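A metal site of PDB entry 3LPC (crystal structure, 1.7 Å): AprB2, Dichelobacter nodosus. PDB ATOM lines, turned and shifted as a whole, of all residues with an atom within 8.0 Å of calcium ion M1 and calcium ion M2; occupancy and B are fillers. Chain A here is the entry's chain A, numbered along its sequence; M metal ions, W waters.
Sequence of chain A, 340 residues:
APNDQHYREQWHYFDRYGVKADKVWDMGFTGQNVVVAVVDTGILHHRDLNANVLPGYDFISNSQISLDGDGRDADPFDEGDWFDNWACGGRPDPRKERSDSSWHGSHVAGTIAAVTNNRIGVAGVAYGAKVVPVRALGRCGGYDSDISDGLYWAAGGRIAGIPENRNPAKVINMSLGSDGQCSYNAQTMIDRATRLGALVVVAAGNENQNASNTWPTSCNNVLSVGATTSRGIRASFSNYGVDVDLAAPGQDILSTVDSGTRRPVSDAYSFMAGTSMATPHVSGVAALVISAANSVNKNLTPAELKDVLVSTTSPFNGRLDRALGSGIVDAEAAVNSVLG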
ATOM      1  N   TYR A  57      22.353 -12.626  15.520  1.00  0.00           N
ATOM      2  CA  TYR A  57      23.169 -11.840  14.592  1.00  0.00           C
ATOM      3  C   TYR A  57      22.422 -10.575  14.226  1.00  0.00           C
ATOM      4  O   TYR A  57      21.194 -10.563  14.248  1.00  0.00           O
ATOM      5  CB  TYR A  57      23.583 -12.648  13.352  1.00  0.00           C
ATOM      6  CG  TYR A  57      24.915 -12.181  12.796  1.00  0.00           C
ATOM      7  CD1 TYR A  57      26.106 -12.723  13.271  1.00  0.00           C
ATOM      8  CD2 TYR A  57      24.985 -11.192  11.819  1.00  0.00           C
ATOM      9  CE1 TYR A  57      27.346 -12.277  12.781  1.00  0.00           C
ATOM     10  CE2 TYR A  57      26.227 -10.736  11.327  1.00  0.00           C
ATOM     11  CZ  TYR A  57      27.395 -11.288  11.817  1.00  0.00           C
ATOM     12  OH  TYR A  57      28.623 -10.873  11.359  1.00  0.00           O
ATOM     13  N   ASP A  58      23.165  -9.501  13.961  1.00  0.00           N
ATOM     14  CA  ASP A  58      22.555  -8.195  13.647  1.00  0.00           C
ATOM     15  C   ASP A  58      22.683  -7.967  12.143  1.00  0.00           C
ATOM     16  O   ASP A  58      23.791  -7.791  11.631  1.00  0.00           O
ATOM     17  CB  ASP A  58      23.287  -7.094  14.446  1.00  0.00           C
ATOM     18  CG  ASP A  58      22.575  -5.761  14.407  1.00  0.00           C
ATOM     19  OD1 ASP A  58      21.847  -5.462  13.432  1.00  0.00           O
ATOM     20  OD2 ASP A  58      22.784  -4.978  15.358  1.00  0.00           O
ATOM     21  N   PHE A  59      21.553  -8.019  11.442  1.00  0.00           N
ATOM     22  CA  PHE A  59      21.478  -7.891   9.998  1.00  0.00           C
ATOM     23  C   PHE A  59      21.222  -6.470   9.521  1.00  0.00           C
ATOM     24  O   PHE A  59      21.138  -6.248   8.328  1.00  0.00           O
ATOM     25  CB  PHE A  59      20.402  -8.829   9.445  1.00  0.00           C
ATOM     26  CG  PHE A  59      20.894 -10.229   9.295  1.00  0.00           C
ATOM     27  CD1 PHE A  59      21.381 -10.689   8.070  1.00  0.00           C
ATOM     28  CD2 PHE A  59      20.931 -11.072  10.408  1.00  0.00           C
ATOM     29  CE1 PHE A  59      21.881 -11.988   7.943  1.00  0.00           C
ATOM     30  CE2 PHE A  59      21.423 -12.377  10.291  1.00  0.00           C
ATOM     31  CZ  PHE A  59      21.910 -12.836   9.066  1.00  0.00           C
ATOM     32  N   ILE A  60      21.120  -5.512  10.445  1.00  0.00           N
ATOM     33  CA  ILE A  60      20.863  -4.130  10.022  1.00  0.00           C
ATOM     34  C   ILE A  60      22.089  -3.547   9.314  1.00  0.00           C
ATOM     35  O   ILE A  60      23.160  -3.437   9.892  1.00  0.00           O
ATOM     36  CB  ILE A  60      20.437  -3.199  11.188  1.00  0.00           C
ATOM     37  CG1 ILE A  60      19.195  -3.744  11.906  1.00  0.00           C
ATOM     38  CG2 ILE A  60      20.116  -1.807  10.622  1.00  0.00           C
ATOM     39  CD1 ILE A  60      18.818  -2.936  13.181  1.00  0.00           C
ATOM     40  N   SER A  61      21.915  -3.160   8.046  1.00  0.00           N
ATOM     41  CA  SER A  61      23.014  -2.703   7.219  1.00  0.00           C
ATOM     42  C   SER A  61      23.364  -1.213   7.371  1.00  0.00           C
ATOM     43  O   SER A  61      24.508  -0.821   7.134  1.00  0.00           O
ATOM     44  CB  SER A  61      22.696  -2.996   5.752  1.00  0.00           C
ATOM     45  OG  SER A  61      22.705  -4.405   5.555  1.00  0.00           O
ATOM     46  N   ASN A  62      22.371  -0.400   7.729  1.00  0.00           N
ATOM     47  CA  ASN A  62      22.508   1.057   7.781  1.00  0.00           C
ATOM     48  C   ASN A  62      22.655   1.502   9.240  1.00  0.00           C
ATOM     49  O   ASN A  62      21.769   1.232  10.062  1.00  0.00           O
ATOM     50  CB  ASN A  62      21.278   1.687   7.120  1.00  0.00           C
ATOM     51  CG  ASN A  62      21.347   3.187   7.025  1.00  0.00           C
ATOM     52  OD1 ASN A  62      22.066   3.848   7.773  1.00  0.00           O
ATOM     53  ND2 ASN A  62      20.590   3.748   6.079  1.00  0.00           N
ATOM     54  N   SER A  63      23.788   2.137   9.562  1.00  0.00           N
ATOM     55  CA  SER A  63      24.071   2.564  10.937  1.00  0.00           C
ATOM     56  C   SER A  63      23.093   3.621  11.458  1.00  0.00           C
ATOM     57  O   SER A  63      22.957   3.791  12.683  1.00  0.00           O
ATOM     58  CB  SER A  63      25.511   3.051  11.071  1.00  0.00           C
ATOM     59  OG  SER A  63      25.747   4.154  10.205  1.00  0.00           O
ATOM     60  N   ILE A  65      19.982   3.323  11.116  1.00  0.00           N
ATOM     61  CA  ILE A  65      18.878   2.514  11.634  1.00  0.00           C
ATOM     62  C   ILE A  65      19.325   1.696  12.856  1.00  0.00           C
ATOM     63  O   ILE A  65      18.587   1.591  13.843  1.00  0.00           O
ATOM     64  CB  ILE A  65      18.296   1.568  10.533  1.00  0.00           C
ATOM     65  CG1 ILE A  65      17.715   2.398   9.374  1.00  0.00           C
ATOM     66  CG2 ILE A  65      17.262   0.593  11.140  1.00  0.00           C
ATOM     67  CD1 ILE A  65      17.320   1.576   8.131  1.00  0.00           C
ATOM     68  N   SER A  66      20.527   1.131  12.788  1.00  0.00           N
ATOM     69  CA  SER A  66      21.023   0.222  13.806  1.00  0.00           C
ATOM     70  C   SER A  66      21.361   0.918  15.119  1.00  0.00           C
ATOM     71  O   SER A  66      21.257   0.318  16.192  1.00  0.00           O
ATOM     72  CB  SER A  66      22.286  -0.490  13.303  1.00  0.00           C
ATOM     73  OG  SER A  66      23.370   0.424  13.187  1.00  0.00           O
ATOM     74  N   LEU A  67      21.793   2.175  15.012  1.00  0.00           N
ATOM     75  CA  LEU A  67      22.225   2.982  16.159  1.00  0.00           C
ATOM     76  C   LEU A  67      23.370   2.330  16.966  1.00  0.00           C
ATOM     77  O   LEU A  67      23.533   2.599  18.152  1.00  0.00           O
ATOM     78  CB  LEU A  67      21.035   3.324  17.067  1.00  0.00           C
ATOM     79  CG  LEU A  67      19.873   4.094  16.397  1.00  0.00           C
ATOM     80  CD1 LEU A  67      18.811   4.453  17.461  1.00  0.00           C
ATOM     81  CD2 LEU A  67      20.345   5.313  15.683  1.00  0.00           C
ATOM     82  N   ASP A  68      24.174   1.497  16.305  1.00  0.00           N
ATOM     83  CA  ASP A  68      25.286   0.856  17.000  1.00  0.00           C
ATOM     84  C   ASP A  68      26.631   1.152  16.304  1.00  0.00           C
ATOM     85  O   ASP A  68      27.643   0.502  16.595  1.00  0.00           O
ATOM     86  CB  ASP A  68      25.029  -0.659  17.126  1.00  0.00           C
ATOM     87  CG  ASP A  68      25.054  -1.389  15.782  1.00  0.00           C
ATOM     88  OD1 ASP A  68      25.355  -0.760  14.740  1.00  0.00           O
ATOM     89  OD2 ASP A  68      24.758  -2.597  15.775  1.00  0.00           O
ATOM     90  N   GLY A  69      26.631   2.087  15.371  1.00  0.00           N
ATOM     91  CA  GLY A  69      27.874   2.588  14.772  1.00  0.00           C
ATOM     92  C   GLY A  69      28.370   1.887  13.534  1.00  0.00           C
ATOM     93  O   GLY A  69      29.327   2.342  12.910  1.00  0.00           O
ATOM     94  N   ASP A  70      27.747   0.764  13.158  1.00  0.00           N
ATOM     95  CA  ASP A  70      28.238  -0.015  12.026  1.00  0.00           C
ATOM     96  C   ASP A  70      27.118  -0.827  11.379  1.00  0.00           C
ATOM     97  O   ASP A  70      25.998  -0.859  11.895  1.00  0.00           O
ATOM     98  CB  ASP A  70      29.438  -0.922  12.430  1.00  0.00           C
ATOM     99  CG  ASP A  70      29.102  -1.979  13.477  1.00  0.00           C
ATOM    100  OD1 ASP A  70      27.928  -2.220  13.804  1.00  0.00           O
ATOM    101  OD2 ASP A  70      30.063  -2.605  14.001  1.00  0.00           O
ATOM    102  N   GLY A  71      27.429  -1.475  10.269  1.00  0.00           N
ATOM    103  CA  GLY A  71      26.490  -2.358   9.587  1.00  0.00           C
ATOM    104  C   GLY A  71      26.363  -3.704  10.263  1.00  0.00           C
ATOM    105  O   GLY A  71      26.357  -3.813  11.502  1.00  0.00           O
ATOM    106  N   ARG A  72      26.242  -4.741   9.452  1.00  0.00           N
ATOM    107  CA  ARG A  72      25.979  -6.067  10.026  1.00  0.00           C
ATOM    108  C   ARG A  72      27.071  -6.456  10.996  1.00  0.00           C
ATOM    109  O   ARG A  72      28.245  -6.194  10.748  1.00  0.00           O
ATOM    110  CB  ARG A  72      25.801  -7.095   8.915  1.00  0.00           C
ATOM    111  CG  ARG A  72      24.610  -6.732   8.022  1.00  0.00           C
ATOM    112  CD  ARG A  72      24.268  -7.881   7.090  1.00  0.00           C
ATOM    113  NE  ARG A  72      23.009  -7.631   6.380  1.00  0.00           N
ATOM    114  CZ  ARG A  72      22.560  -8.365   5.365  1.00  0.00           C
ATOM    115  NH1 ARG A  72      23.290  -9.381   4.902  1.00  0.00           N
ATOM    116  NH2 ARG A  72      21.398  -8.063   4.789  1.00  0.00           N
ATOM    117  N   ASP A  73      26.674  -7.058  12.119  1.00  0.00           N
ATOM    118  CA  ASP A  73      27.636  -7.373  13.191  1.00  0.00           C
ATOM    119  C   ASP A  73      27.105  -8.493  14.050  1.00  0.00           C
ATOM    120  O   ASP A  73      25.921  -8.811  14.007  1.00  0.00           O
ATOM    121  CB  ASP A  73      27.957  -6.123  14.040  1.00  0.00           C
ATOM    122  CG  ASP A  73      26.790  -5.698  14.925  1.00  0.00           C
ATOM    123  OD1 ASP A  73      25.970  -4.854  14.477  1.00  0.00           O
ATOM    124  OD2 ASP A  73      26.646  -6.206  16.057  1.00  0.00           O
ATOM    125  N   ALA A  74      27.982  -9.076  14.878  1.00  0.00           N
ATOM    126  CA  ALA A  74      27.621 -10.268  15.646  1.00  0.00           C
ATOM    127  C   ALA A  74      26.760 -10.047  16.877  1.00  0.00           C
ATOM    128  O   ALA A  74      26.413 -11.030  17.562  1.00  0.00           O
ATOM    129  CB  ALA A  74      28.879 -11.056  15.995  1.00  0.00           C
ATOM    130  N   ASP A  75      26.419  -8.787  17.179  1.00  0.00           N
ATOM    131  CA  ASP A  75      25.715  -8.466  18.423  1.00  0.00           C
ATOM    132  C   ASP A  75      24.319  -7.917  18.158  1.00  0.00           C
ATOM    133  O   ASP A  75      24.182  -6.756  17.754  1.00  0.00           O
ATOM    134  CB  ASP A  75      26.509  -7.441  19.242  1.00  0.00           C
ATOM    135  CG  ASP A  75      25.857  -7.139  20.587  1.00  0.00           C
ATOM    136  OD1 ASP A  75      24.798  -7.736  20.902  1.00  0.00           O
ATOM    137  OD2 ASP A  75      26.404  -6.290  21.337  1.00  0.00           O
ATOM    138  N   PRO A  76      23.275  -8.750  18.374  1.00  0.00           N
ATOM    139  CA  PRO A  76      21.910  -8.330  18.023  1.00  0.00           C
ATOM    140  C   PRO A  76      21.215  -7.577  19.170  1.00  0.00           C
ATOM    141  O   PRO A  76      19.989  -7.578  19.262  1.00  0.00           O
ATOM    142  CB  PRO A  76      21.221  -9.679  17.770  1.00  0.00           C
ATOM    143  CG  PRO A  76      21.826 -10.570  18.807  1.00  0.00           C
ATOM    144  CD  PRO A  76      23.305 -10.162  18.813  1.00  0.00           C
ATOM    145  N   PHE A  77      22.012  -6.937  20.036  1.00  0.00           N
ATOM    146  CA  PHE A  77      21.446  -6.106  21.088  1.00  0.00           C
ATOM    147  C   PHE A  77      20.474  -5.065  20.500  1.00  0.00           C
ATOM    148  O   PHE A  77      20.756  -4.422  19.490  1.00  0.00           O
ATOM    149  CB  PHE A  77      22.559  -5.418  21.897  1.00  0.00           C
ATOM    150  CG  PHE A  77      22.060  -4.719  23.122  1.00  0.00           C
ATOM    151  CD1 PHE A  77      21.606  -5.452  24.218  1.00  0.00           C
ATOM    152  CD2 PHE A  77      22.020  -3.319  23.180  1.00  0.00           C
ATOM    153  CE1 PHE A  77      21.116  -4.804  25.346  1.00  0.00           C
ATOM    154  CE2 PHE A  77      21.538  -2.671  24.314  1.00  0.00           C
ATOM    155  CZ  PHE A  77      21.084  -3.420  25.391  1.00  0.00           C
ATOM    156  N   ASP A  78      19.324  -4.903  21.149  1.00  0.00           N
ATOM    157  CA  ASP A  78      18.362  -3.884  20.727  1.00  0.00           C
ATOM    158  C   ASP A  78      18.843  -2.567  21.356  1.00  0.00           C
ATOM    159  O   ASP A  78      18.665  -2.342  22.544  1.00  0.00           O
ATOM    160  CB  ASP A  78      16.972  -4.272  21.238  1.00  0.00           C
ATOM    161  CG  ASP A  78      15.871  -3.310  20.782  1.00  0.00           C
ATOM    162  OD1 ASP A  78      16.207  -2.227  20.258  1.00  0.00           O
ATOM    163  OD2 ASP A  78      14.683  -3.634  20.950  1.00  0.00           O
ATOM    164  N   GLU A  79      19.425  -1.700  20.526  1.00  0.00           N
ATOM    165  CA  GLU A  79      19.959  -0.428  21.008  1.00  0.00           C
ATOM    166  C   GLU A  79      18.842   0.500  21.465  1.00  0.00           C
ATOM    167  O   GLU A  79      19.114   1.479  22.181  1.00  0.00           O
ATOM    168  CB  GLU A  79      20.750   0.274  19.902  1.00  0.00           C
ATOM    169  CG  GLU A  79      21.865  -0.565  19.293  1.00  0.00           C
ATOM    170  CD  GLU A  79      22.985  -0.903  20.245  1.00  0.00           C
ATOM    171  OE1 GLU A  79      23.234  -0.111  21.191  1.00  0.00           O
ATOM    172  OE2 GLU A  79      23.657  -1.951  20.036  1.00  0.00           O
ATOM    173  N   ARG A 135      18.400  -9.583  14.541  1.00  0.00           N
ATOM    174  CA  ARG A 135      18.079  -8.159  14.559  1.00  0.00           C
ATOM    175  C   ARG A 135      18.054  -7.619  13.138  1.00  0.00           C
ATOM    176  O   ARG A 135      19.079  -7.585  12.453  1.00  0.00           O
ATOM    177  CB  ARG A 135      19.064  -7.381  15.414  1.00  0.00           C
ATOM    178  CG  ARG A 135      18.737  -5.874  15.491  1.00  0.00           C
ATOM    179  CD  ARG A 135      19.558  -5.166  16.553  1.00  0.00           C
ATOM    180  NE  ARG A 135      19.058  -3.817  16.820  1.00  0.00           N
ATOM    181  CZ  ARG A 135      19.791  -2.693  16.689  1.00  0.00           C
ATOM    182  NH1 ARG A 135      21.038  -2.730  16.242  1.00  0.00           N
ATOM    183  NH2 ARG A 135      19.261  -1.513  17.013  1.00  0.00           N
HETATM  184 CA    CA M   1      24.704  -4.721  16.699  1.00  0.00          CA
HETATM  185 CA    CA M   2      25.734  -2.800  13.435  1.00  0.00          CA
HETATM  186  O   HOH W   1      23.226  -3.908  18.410  1.00  0.00           O
HETATM  187  O   HOH W   2      26.387  -3.932  18.140  1.00  0.00           O
HETATM  188  O   HOH W   3      23.645  -3.339  12.576  1.00  0.00           O
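The backbone carbonyl oxygen of Asp 70 lies close to the side-chain hydroxyl of Ser 66, 3.2 Å away. The side-chain hydroxyl (OG) of Ser 66 sits close to the backbone NH (N) of Asp 68 (3.4 Å). The guanidinium group (NH1) of Arg 135 sits close to the side-chain carboxylate (OD2) of Asp 68 (3.8 Å). N of Phe 77 is in hydrogen-bond range of OD1 of Asp 75, 3.0 Å away. The guanidinium group (NH1) of Arg 135 sits close to the side-chain carboxylate (OD2) of Asp 58 (3.0 Å). OD1 of Asp 58 is in hydrogen-bond range of N of Ile 60, at 3.1 Å.
The nearest printed residue that does not touch calcium ion M1 is Arg 135 (4.2 Å).
Of the 23 residues printed, 4 come within 4 Å of calcium ion M2. The nearest printed residue that does not touch calcium ion M2 is Ser 66 (4.01 Å).
Calcium ion M1 is bound by OD2 of Asp 68 (2.3 Å). Calcium ion M1 is bound by O of Asp 75, 2.4 Å away. Calcium ion M1 is bound by water W2. OD2 of Asp 58 is bound to calcium ion M1, 2.4 Å away. Water W1 binds calcium ion M1 (2.4 Å). OD2 of Asp 73 binds calcium ion M1, 2.5 Å away. OD1 of Asp 73 binds calcium ion M1 (2.6 Å). Calcium ion M1 has seven donor atoms within binding distance.
Calcium ion M2 is bound by O of Gly 71 (2.3 Å), OD1 of Asp 70 (2.3 Å), OD1 of Asp 73 (2.3 Å), water W3 (2.3 Å), OD1 of Asp 68 (2.5 Å), O of Asp 70 (2.5 Å) and OD2 of Asp 68 (2.5 Å). Calcium ion M2 has seven donor atoms within binding distance.
Water W1 lies within hydrogen-bond range of the side-chain carboxylate (OE2) of Glu 79, the backbone carbonyl oxygen (O) of Phe 77 and the guanidinium group (NH1) of Arg 135. Water W3 lies within hydrogen-bond range of the backbone carbonyl oxygen of Ile 60 and the side-chain carboxylate of Asp 58.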
